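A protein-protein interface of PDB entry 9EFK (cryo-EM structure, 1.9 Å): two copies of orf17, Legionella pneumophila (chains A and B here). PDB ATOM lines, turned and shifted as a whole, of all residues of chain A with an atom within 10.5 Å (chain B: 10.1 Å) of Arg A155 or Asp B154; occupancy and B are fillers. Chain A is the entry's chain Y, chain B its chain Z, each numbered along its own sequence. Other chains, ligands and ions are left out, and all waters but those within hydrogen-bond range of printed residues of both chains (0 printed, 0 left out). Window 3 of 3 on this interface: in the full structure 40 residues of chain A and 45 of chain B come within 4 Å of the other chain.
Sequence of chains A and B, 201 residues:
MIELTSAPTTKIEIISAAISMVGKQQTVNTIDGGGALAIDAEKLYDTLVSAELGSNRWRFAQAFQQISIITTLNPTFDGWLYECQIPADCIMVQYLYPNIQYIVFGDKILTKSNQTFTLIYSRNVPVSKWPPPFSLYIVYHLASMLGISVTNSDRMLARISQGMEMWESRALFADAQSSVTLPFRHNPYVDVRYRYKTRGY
Asn B152 touches its own counterpart, Asn A152. Ser A153 touches Asp B154, but with the chains exchanged Asp A154 does not touch Ser B153 (10.1 Å). Arg A159 touches Leu B157, but with the chains exchanged Leu A157 does not touch Arg B159 (14.1 Å). Arg A159 touches Ala B158, but with the chains exchanged Ala A158 does not touch Arg B159 (13.3 Å). Positions printed for both chains: 147, 151, 152, 153, 154, 155, 156, 157, 158, 159, 160 and 161.
Arg A155 touches just one residue of chain B: Asp B154. Asp B154 touches just these residues of chain A: Ser A153, Arg A155, Met A156 and Arg A159. Ser A153 touches one residue of chain B. Of the printed residues of chain B, Ile A160 touches Ile B148 (3.99 Å). Of the printed residues of chain B, Met A156 touches Ile B148, Ser B153 and Asp B154. Of the printed residues of chain B, Asn A152 touches Asn B152 (3.3 Å). Gln A162 touches none of the printed residues of chain B. The nearest residue of chain B that does not touch Arg A155 is Arg B155 (5.5 Å). The nearest printed residue of chain A that does not touch Asp B154 is Asp A154 (5.9 Å). The nearest printed residue of chain A that does not touch Asn B152 is Met A156 (4.01 Å).
The side-chain amide oxygen of Asn A152 sits at hydrogen-bond distance from the side-chain amide nitrogen of Asn B152. The side-chain hydroxyl of Ser A153 sits at hydrogen-bond distance from the side-chain carboxylate of Asp B154 (2.8 Å). The guanidinium group of Arg A155 lies within salt-bridge range of the side-chain carboxylate of Asp B154, 3.3 Å away. The backbone NH (N) of Met A156 lies within hydrogen-bond range of the side-chain carboxylate (OD1) of Asp B154. OD1 of Asp B154 lies within salt-bridge range of NH1 of Arg A159, at 3.4 Å.
Printed residues of chain B that touch a printed residue of chain A: Ile B148, Asn B152, Ser B153, Asp B154, Leu B157 and Ala B158. Hydrophobic or aromatic side chains of chain B that line the printed part of chain A: Ile B148, Leu B157 and Ala B158. Hydrophobic or aromatic side chains of chain A that line the printed part of chain B: Met A156 and Ile A160.
Among the printed residues, merely in contact across the chains: Met A21 with Ile B148, Met A156 with Ile B148, Met A156 with Ser B153, Arg A159 with Leu B157, Arg A159 with Ala B158 and Ile A160 with Ile B148.
The side-chain hydroxyl (OG) of Ser A153 lies within hydrogen-bond range of the backbone NH (N) of Arg A155 (3.1 Å). The side-chain hydroxyl (OG) of Ser A153 lies within hydrogen-bond range of the backbone NH (N) of Met A156. O of Gly B147 lies within hydrogen-bond range of N of Asn B152 (3.1 Å). The side-chain hydroxyl of Thr B151 sits close to the backbone NH of Ser B153. The backbone NH (N) of Arg B155 sits close to the side-chain hydroxyl (OG) of Ser B153 (3.4 Å). O of Leu B157 is in hydrogen-bond range of OG of Ser B161.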
ATOM      1  N   MET A  21      -6.422  -6.767   6.449  1.00  0.00           N
ATOM      2  CA  MET A  21      -6.868  -8.088   6.035  1.00  0.00           C
ATOM      3  C   MET A  21      -6.067  -8.670   4.877  1.00  0.00           C
ATOM      4  O   MET A  21      -6.246  -9.848   4.568  1.00  0.00           O
ATOM      5  CB  MET A  21      -8.352  -8.054   5.675  1.00  0.00           C
ATOM      6  CG  MET A  21      -9.254  -7.725   6.851  1.00  0.00           C
ATOM      7  SD  MET A  21      -8.951  -8.748   8.307  1.00  0.00           S
ATOM      8  CE  MET A  21      -9.358 -10.370   7.678  1.00  0.00           C
ATOM      9  N   VAL A  22      -5.195  -7.899   4.230  1.00  0.00           N
ATOM     10  CA  VAL A  22      -4.252  -8.493   3.288  1.00  0.00           C
ATOM     11  C   VAL A  22      -2.940  -8.758   4.009  1.00  0.00           C
ATOM     12  O   VAL A  22      -1.923  -9.061   3.380  1.00  0.00           O
ATOM     13  CB  VAL A  22      -4.023  -7.621   2.038  1.00  0.00           C
ATOM     14  CG1 VAL A  22      -4.948  -8.046   0.938  1.00  0.00           C
ATOM     15  CG2 VAL A  22      -4.210  -6.159   2.346  1.00  0.00           C
ATOM     16  N   GLY A 147      -5.293  -8.043  -2.670  1.00  0.00           N
ATOM     17  CA  GLY A 147      -4.539  -9.274  -2.541  1.00  0.00           C
ATOM     18  C   GLY A 147      -4.200  -9.942  -3.849  1.00  0.00           C
ATOM     19  O   GLY A 147      -3.376 -10.858  -3.854  1.00  0.00           O
ATOM     20  N   THR A 151      -0.867 -10.498  -1.993  1.00  0.00           N
ATOM     21  CA  THR A 151      -0.960 -11.673  -1.135  1.00  0.00           C
ATOM     22  C   THR A 151       0.047 -12.726  -1.585  1.00  0.00           C
ATOM     23  O   THR A 151       0.116 -13.060  -2.770  1.00  0.00           O
ATOM     24  CB  THR A 151      -2.376 -12.245  -1.150  1.00  0.00           C
ATOM     25  OG1 THR A 151      -3.258 -11.344  -0.475  1.00  0.00           O
ATOM     26  CG2 THR A 151      -2.425 -13.592  -0.455  1.00  0.00           C
ATOM     27  N   ASN A 152       0.826 -13.247  -0.636  1.00  0.00           N
ATOM     28  CA  ASN A 152       1.894 -14.180  -0.983  1.00  0.00           C
ATOM     29  C   ASN A 152       1.343 -15.528  -1.433  1.00  0.00           C
ATOM     30  O   ASN A 152       1.755 -16.061  -2.469  1.00  0.00           O
ATOM     31  CB  ASN A 152       2.840 -14.366   0.205  1.00  0.00           C
ATOM     32  CG  ASN A 152       3.338 -13.053   0.775  1.00  0.00           C
ATOM     33  OD1 ASN A 152       3.458 -12.901   1.988  1.00  0.00           O
ATOM     34  ND2 ASN A 152       3.630 -12.100  -0.094  1.00  0.00           N
ATOM     35  N   SER A 153       0.407 -16.092  -0.680  1.00  0.00           N
ATOM     36  CA  SER A 153      -0.027 -17.469  -0.869  1.00  0.00           C
ATOM     37  C   SER A 153      -1.372 -17.531  -1.579  1.00  0.00           C
ATOM     38  O   SER A 153      -2.279 -16.752  -1.281  1.00  0.00           O
ATOM     39  CB  SER A 153      -0.124 -18.186   0.477  1.00  0.00           C
ATOM     40  OG  SER A 153      -0.789 -19.427   0.352  1.00  0.00           O
ATOM     41  N   ASP A 154      -1.497 -18.469  -2.519  1.00  0.00           N
ATOM     42  CA  ASP A 154      -2.788 -18.689  -3.162  1.00  0.00           C
ATOM     43  C   ASP A 154      -3.817 -19.201  -2.166  1.00  0.00           C
ATOM     44  O   ASP A 154      -4.999 -18.854  -2.253  1.00  0.00           O
ATOM     45  CB  ASP A 154      -2.647 -19.667  -4.325  1.00  0.00           C
ATOM     46  CG  ASP A 154      -1.957 -19.056  -5.522  1.00  0.00           C
ATOM     47  OD1 ASP A 154      -1.971 -17.817  -5.653  1.00  0.00           O
ATOM     48  OD2 ASP A 154      -1.409 -19.820  -6.339  1.00  0.00           O
ATOM     49  N   ARG A 155      -3.388 -20.035  -1.218  1.00  0.00           N
ATOM     50  CA  ARG A 155      -4.306 -20.524  -0.197  1.00  0.00           C
ATOM     51  C   ARG A 155      -4.816 -19.390   0.680  1.00  0.00           C
ATOM     52  O   ARG A 155      -5.984 -19.381   1.077  1.00  0.00           O
ATOM     53  CB  ARG A 155      -3.624 -21.595   0.649  1.00  0.00           C
ATOM     54  CG  ARG A 155      -4.183 -22.979   0.425  1.00  0.00           C
ATOM     55  CD  ARG A 155      -3.097 -23.997   0.147  1.00  0.00           C
ATOM     56  NE  ARG A 155      -2.178 -24.157   1.267  1.00  0.00           N
ATOM     57  CZ  ARG A 155      -0.914 -23.757   1.260  1.00  0.00           C
ATOM     58  NH1 ARG A 155      -0.382 -23.165   0.204  1.00  0.00           N
ATOM     59  NH2 ARG A 155      -0.162 -23.965   2.337  1.00  0.00           N
ATOM     60  N   MET A 156      -3.949 -18.431   1.004  1.00  0.00           N
ATOM     61  CA  MET A 156      -4.381 -17.293   1.804  1.00  0.00           C
ATOM     62  C   MET A 156      -5.358 -16.414   1.033  1.00  0.00           C
ATOM     63  O   MET A 156      -6.343 -15.931   1.599  1.00  0.00           O
ATOM     64  CB  MET A 156      -3.170 -16.484   2.260  1.00  0.00           C
ATOM     65  CG  MET A 156      -3.516 -15.314   3.156  1.00  0.00           C
ATOM     66  SD  MET A 156      -4.389 -15.818   4.648  1.00  0.00           S
ATOM     67  CE  MET A 156      -3.081 -16.645   5.539  1.00  0.00           C
ATOM     68  N   LEU A 157      -5.103 -16.195  -0.257  1.00  0.00           N
ATOM     69  CA  LEU A 157      -6.022 -15.394  -1.057  1.00  0.00           C
ATOM     70  C   LEU A 157      -7.372 -16.080  -1.189  1.00  0.00           C
ATOM     71  O   LEU A 157      -8.412 -15.416  -1.188  1.00  0.00           O
ATOM     72  CB  LEU A 157      -5.426 -15.122  -2.436  1.00  0.00           C
ATOM     73  CG  LEU A 157      -5.578 -13.714  -3.014  1.00  0.00           C
ATOM     74  CD1 LEU A 157      -5.532 -13.769  -4.519  1.00  0.00           C
ATOM     75  CD2 LEU A 157      -6.835 -13.008  -2.546  1.00  0.00           C
ATOM     76  N   ALA A 158      -7.376 -17.408  -1.307  1.00  0.00           N
ATOM     77  CA  ALA A 158      -8.635 -18.139  -1.375  1.00  0.00           C
ATOM     78  C   ALA A 158      -9.459 -17.933  -0.114  1.00  0.00           C
ATOM     79  O   ALA A 158     -10.682 -17.786  -0.183  1.00  0.00           O
ATOM     80  CB  ALA A 158      -8.371 -19.624  -1.603  1.00  0.00           C
ATOM     81  N   ARG A 159      -8.808 -17.921   1.050  1.00  0.00           N
ATOM     82  CA  ARG A 159      -9.541 -17.729   2.296  1.00  0.00           C
ATOM     83  C   ARG A 159     -10.089 -16.315   2.410  1.00  0.00           C
ATOM     84  O   ARG A 159     -11.177 -16.111   2.958  1.00  0.00           O
ATOM     85  CB  ARG A 159      -8.650 -18.060   3.488  1.00  0.00           C
ATOM     86  CG  ARG A 159      -8.286 -19.524   3.569  1.00  0.00           C
ATOM     87  CD  ARG A 159      -7.867 -19.906   4.967  1.00  0.00           C
ATOM     88  NE  ARG A 159      -7.250 -21.226   5.014  1.00  0.00           N
ATOM     89  CZ  ARG A 159      -5.966 -21.459   4.776  1.00  0.00           C
ATOM     90  NH1 ARG A 159      -5.136 -20.483   4.447  1.00  0.00           N
ATOM     91  NH2 ARG A 159      -5.504 -22.701   4.872  1.00  0.00           N
ATOM     92  N   ILE A 160      -9.349 -15.325   1.914  1.00  0.00           N
ATOM     93  CA  ILE A 160      -9.867 -13.961   1.897  1.00  0.00           C
ATOM     94  C   ILE A 160     -11.091 -13.872   0.997  1.00  0.00           C
ATOM     95  O   ILE A 160     -12.091 -13.238   1.346  1.00  0.00           O
ATOM     96  CB  ILE A 160      -8.769 -12.972   1.469  1.00  0.00           C
ATOM     97  CG1 ILE A 160      -7.703 -12.863   2.558  1.00  0.00           C
ATOM     98  CG2 ILE A 160      -9.358 -11.609   1.179  1.00  0.00           C
ATOM     99  CD1 ILE A 160      -6.506 -12.052   2.152  1.00  0.00           C
ATOM    100  N   SER A 161     -11.036 -14.509  -0.173  1.00  0.00           N
ATOM    101  CA  SER A 161     -12.199 -14.534  -1.051  1.00  0.00           C
ATOM    102  C   SER A 161     -13.357 -15.297  -0.427  1.00  0.00           C
ATOM    103  O   SER A 161     -14.519 -14.957  -0.664  1.00  0.00           O
ATOM    104  CB  SER A 161     -11.833 -15.146  -2.400  1.00  0.00           C
ATOM    105  OG  SER A 161     -10.849 -14.372  -3.055  1.00  0.00           O
ATOM    106  N   GLN A 162     -13.067 -16.341   0.353  1.00  0.00           N
ATOM    107  CA  GLN A 162     -14.129 -17.056   1.052  1.00  0.00           C
ATOM    108  C   GLN A 162     -14.818 -16.160   2.069  1.00  0.00           C
ATOM    109  O   GLN A 162     -16.041 -16.208   2.219  1.00  0.00           O
ATOM    110  CB  GLN A 162     -13.569 -18.302   1.736  1.00  0.00           C
ATOM    111  CG  GLN A 162     -13.245 -19.434   0.791  1.00  0.00           C
ATOM    112  CD  GLN A 162     -12.559 -20.593   1.486  1.00  0.00           C
ATOM    113  OE1 GLN A 162     -12.705 -20.784   2.693  1.00  0.00           O
ATOM    114  NE2 GLN A 162     -11.799 -21.368   0.726  1.00  0.00           N
ATOM    115  N   GLY A 163     -14.044 -15.346   2.785  1.00  0.00           N
ATOM    116  CA  GLY A 163     -14.637 -14.387   3.699  1.00  0.00           C
ATOM    117  C   GLY A 163     -15.473 -13.340   2.995  1.00  0.00           C
ATOM    118  O   GLY A 163     -16.480 -12.882   3.535  1.00  0.00           O
ATOM    119  N   SER B 144      -9.334 -16.201  13.907  1.00  0.00           N
ATOM    120  CA  SER B 144      -9.230 -16.472  12.480  1.00  0.00           C
ATOM    121  C   SER B 144      -8.811 -15.226  11.711  1.00  0.00           C
ATOM    122  O   SER B 144      -7.973 -15.301  10.809  1.00  0.00           O
ATOM    123  CB  SER B 144     -10.562 -17.007  11.962  1.00  0.00           C
ATOM    124  OG  SER B 144     -10.556 -17.113  10.556  1.00  0.00           O
ATOM    125  N   LEU B 146      -7.132 -12.748  12.997  1.00  0.00           N
ATOM    126  CA  LEU B 146      -5.748 -12.485  13.372  1.00  0.00           C
ATOM    127  C   LEU B 146      -4.783 -13.368  12.598  1.00  0.00           C
ATOM    128  O   LEU B 146      -3.655 -12.955  12.319  1.00  0.00           O
ATOM    129  CB  LEU B 146      -5.554 -12.683  14.873  1.00  0.00           C
ATOM    130  CG  LEU B 146      -6.250 -11.685  15.798  1.00  0.00           C
ATOM    131  CD1 LEU B 146      -5.929 -11.989  17.248  1.00  0.00           C
ATOM    132  CD2 LEU B 146      -5.843 -10.270  15.449  1.00  0.00           C
ATOM    133  N   GLY B 147      -5.197 -14.588  12.257  1.00  0.00           N
ATOM    134  CA  GLY B 147      -4.361 -15.429  11.421  1.00  0.00           C
ATOM    135  C   GLY B 147      -4.116 -14.825  10.053  1.00  0.00           C
ATOM    136  O   GLY B 147      -3.006 -14.888   9.525  1.00  0.00           O
ATOM    137  N   ILE B 148      -5.152 -14.235   9.459  1.00  0.00           N
ATOM    138  CA  ILE B 148      -5.001 -13.601   8.155  1.00  0.00           C
ATOM    139  C   ILE B 148      -4.187 -12.318   8.271  1.00  0.00           C
ATOM    140  O   ILE B 148      -3.269 -12.071   7.484  1.00  0.00           O
ATOM    141  CB  ILE B 148      -6.381 -13.338   7.528  1.00  0.00           C
ATOM    142  CG1 ILE B 148      -7.099 -14.657   7.253  1.00  0.00           C
ATOM    143  CG2 ILE B 148      -6.242 -12.537   6.258  1.00  0.00           C
ATOM    144  CD1 ILE B 148      -8.462 -14.486   6.649  1.00  0.00           C
ATOM    145  N   SER B 149      -4.501 -11.489   9.265  1.00  0.00           N
ATOM    146  CA  SER B 149      -3.909 -10.160   9.338  1.00  0.00           C
ATOM    147  C   SER B 149      -2.478 -10.169   9.858  1.00  0.00           C
ATOM    148  O   SER B 149      -1.689  -9.305   9.473  1.00  0.00           O
ATOM    149  CB  SER B 149      -4.769  -9.248  10.211  1.00  0.00           C
ATOM    150  OG  SER B 149      -4.704  -9.622  11.571  1.00  0.00           O
ATOM    151  N   VAL B 150      -2.118 -11.111  10.727  1.00  0.00           N
ATOM    152  CA  VAL B 150      -0.820 -11.038  11.390  1.00  0.00           C
ATOM    153  C   VAL B 150       0.064 -12.237  11.068  1.00  0.00           C
ATOM    154  O   VAL B 150       1.178 -12.070  10.565  1.00  0.00           O
ATOM    155  CB  VAL B 150      -0.988 -10.891  12.912  1.00  0.00           C
ATOM    156  CG1 VAL B 150       0.362 -10.950  13.591  1.00  0.00           C
ATOM    157  CG2 VAL B 150      -1.685  -9.588  13.239  1.00  0.00           C
ATOM    158  N   THR B 151      -0.408 -13.449  11.368  1.00  0.00           N
ATOM    159  CA  THR B 151       0.478 -14.609  11.310  1.00  0.00           C
ATOM    160  C   THR B 151       0.882 -14.959   9.885  1.00  0.00           C
ATOM    161  O   THR B 151       1.979 -15.483   9.670  1.00  0.00           O
ATOM    162  CB  THR B 151      -0.175 -15.822  11.973  1.00  0.00           C
ATOM    163  OG1 THR B 151      -1.166 -16.371  11.101  1.00  0.00           O
ATOM    164  CG2 THR B 151      -0.827 -15.434  13.286  1.00  0.00           C
ATOM    165  N   ASN B 152       0.014 -14.693   8.908  1.00  0.00           N
ATOM    166  CA  ASN B 152       0.264 -15.024   7.505  1.00  0.00           C
ATOM    167  C   ASN B 152       0.512 -16.518   7.318  1.00  0.00           C
ATOM    168  O   ASN B 152       1.272 -16.930   6.443  1.00  0.00           O
ATOM    169  CB  ASN B 152       1.436 -14.211   6.945  1.00  0.00           C
ATOM    170  CG  ASN B 152       1.459 -14.185   5.434  1.00  0.00           C
ATOM    171  OD1 ASN B 152       0.423 -14.048   4.790  1.00  0.00           O
ATOM    172  ND2 ASN B 152       2.644 -14.322   4.860  1.00  0.00           N
ATOM    173  N   SER B 153      -0.128 -17.347   8.134  1.00  0.00           N
ATOM    174  CA  SER B 153       0.100 -18.784   8.136  1.00  0.00           C
ATOM    175  C   SER B 153      -1.137 -19.496   7.612  1.00  0.00           C
ATOM    176  O   SER B 153      -2.207 -19.413   8.221  1.00  0.00           O
ATOM    177  CB  SER B 153       0.447 -19.274   9.542  1.00  0.00           C
ATOM    178  OG  SER B 153       0.580 -20.680   9.575  1.00  0.00           O
ATOM    179  N   ASP B 154      -0.989 -20.190   6.482  1.00  0.00           N
ATOM    180  CA  ASP B 154      -2.085 -21.007   5.972  1.00  0.00           C
ATOM    181  C   ASP B 154      -2.388 -22.156   6.918  1.00  0.00           C
ATOM    182  O   ASP B 154      -3.542 -22.575   7.052  1.00  0.00           O
ATOM    183  CB  ASP B 154      -1.743 -21.550   4.586  1.00  0.00           C
ATOM    184  CG  ASP B 154      -1.379 -20.463   3.606  1.00  0.00           C
ATOM    185  OD1 ASP B 154      -2.045 -19.409   3.610  1.00  0.00           O
ATOM    186  OD2 ASP B 154      -0.425 -20.664   2.830  1.00  0.00           O
ATOM    187  N   ARG B 155      -1.354 -22.691   7.566  1.00  0.00           N
ATOM    188  CA  ARG B 155      -1.539 -23.789   8.503  1.00  0.00           C
ATOM    189  C   ARG B 155      -2.430 -23.376   9.665  1.00  0.00           C
ATOM    190  O   ARG B 155      -3.342 -24.114  10.048  1.00  0.00           O
ATOM    191  CB  ARG B 155      -0.177 -24.258   9.005  1.00  0.00           C
ATOM    192  CG  ARG B 155      -0.201 -25.455   9.918  1.00  0.00           C
ATOM    193  CD  ARG B 155       1.163 -25.624  10.553  1.00  0.00           C
ATOM    194  NE  ARG B 155       1.535 -27.023  10.701  1.00  0.00           N
ATOM    195  CZ  ARG B 155       2.102 -27.748   9.748  1.00  0.00           C
ATOM    196  NH1 ARG B 155       2.361 -27.238   8.555  1.00  0.00           N
ATOM    197  NH2 ARG B 155       2.416 -29.015   9.997  1.00  0.00           N
ATOM    198  N   MET B 156      -2.190 -22.191  10.227  1.00  0.00           N
ATOM    199  CA  MET B 156      -2.999 -21.714  11.343  1.00  0.00           C
ATOM    200  C   MET B 156      -4.450 -21.516  10.936  1.00  0.00           C
ATOM    201  O   MET B 156      -5.365 -21.843  11.698  1.00  0.00           O
ATOM    202  CB  MET B 156      -2.416 -20.414  11.887  1.00  0.00           C
ATOM    203  CG  MET B 156      -1.087 -20.589  12.578  1.00  0.00           C
ATOM    204  SD  MET B 156      -1.271 -21.416  14.161  1.00  0.00           S
ATOM    205  CE  MET B 156      -2.174 -20.170  15.068  1.00  0.00           C
ATOM    206  N   LEU B 157      -4.682 -20.971   9.743  1.00  0.00           N
ATOM    207  CA  LEU B 157      -6.050 -20.754   9.287  1.00  0.00           C
ATOM    208  C   LEU B 157      -6.804 -22.068   9.152  1.00  0.00           C
ATOM    209  O   LEU B 157      -7.986 -22.149   9.495  1.00  0.00           O
ATOM    210  CB  LEU B 157      -6.047 -20.002   7.961  1.00  0.00           C
ATOM    211  CG  LEU B 157      -6.254 -18.492   8.037  1.00  0.00           C
ATOM    212  CD1 LEU B 157      -7.578 -18.176   8.706  1.00  0.00           C
ATOM    213  CD2 LEU B 157      -5.116 -17.851   8.784  1.00  0.00           C
ATOM    214  N   ALA B 158      -6.136 -23.107   8.652  1.00  0.00           N
ATOM    215  CA  ALA B 158      -6.788 -24.404   8.518  1.00  0.00           C
ATOM    216  C   ALA B 158      -7.155 -24.982   9.879  1.00  0.00           C
ATOM    217  O   ALA B 158      -8.224 -25.581  10.037  1.00  0.00           O
ATOM    218  CB  ALA B 158      -5.884 -25.361   7.748  1.00  0.00           C
ATOM    219  N   ARG B 159      -6.285 -24.808  10.873  1.00  0.00           N
ATOM    220  CA  ARG B 159      -6.532 -25.388  12.187  1.00  0.00           C
ATOM    221  C   ARG B 159      -7.639 -24.660  12.940  1.00  0.00           C
ATOM    222  O   ARG B 159      -8.347 -25.278  13.740  1.00  0.00           O
ATOM    223  CB  ARG B 159      -5.233 -25.398  12.992  1.00  0.00           C
ATOM    224  CG  ARG B 159      -4.309 -26.539  12.610  1.00  0.00           C
ATOM    225  CD  ARG B 159      -2.866 -26.113  12.441  1.00  0.00           C
ATOM    226  NE  ARG B 159      -2.121 -26.076  13.691  1.00  0.00           N
ATOM    227  CZ  ARG B 159      -1.125 -26.894  14.002  1.00  0.00           C
ATOM    228  NH1 ARG B 159      -0.735 -27.853  13.184  1.00  0.00           N
ATOM    229  NH2 ARG B 159      -0.501 -26.739  15.163  1.00  0.00           N
ATOM    230  N   ILE B 160      -7.818 -23.364  12.695  1.00  0.00           N
ATOM    231  CA  ILE B 160      -8.834 -22.607  13.416  1.00  0.00           C
ATOM    232  C   ILE B 160     -10.214 -22.794  12.796  1.00  0.00           C
ATOM    233  O   ILE B 160     -11.229 -22.679  13.489  1.00  0.00           O
ATOM    234  CB  ILE B 160      -8.436 -21.121  13.467  1.00  0.00           C
ATOM    235  CG1 ILE B 160      -7.114 -20.950  14.206  1.00  0.00           C
ATOM    236  CG2 ILE B 160      -9.500 -20.286  14.146  1.00  0.00           C
ATOM    237  CD1 ILE B 160      -6.569 -19.550  14.149  1.00  0.00           C
ATOM    238  N   SER B 161     -10.276 -23.127  11.505  1.00  0.00           N
ATOM    239  CA  SER B 161     -11.543 -23.091  10.779  1.00  0.00           C
ATOM    240  C   SER B 161     -12.557 -24.079  11.341  1.00  0.00           C
ATOM    241  O   SER B 161     -13.754 -23.779  11.397  1.00  0.00           O
ATOM    242  CB  SER B 161     -11.301 -23.364   9.298  1.00  0.00           C
ATOM    243  OG  SER B 161     -10.685 -22.252   8.682  1.00  0.00           O
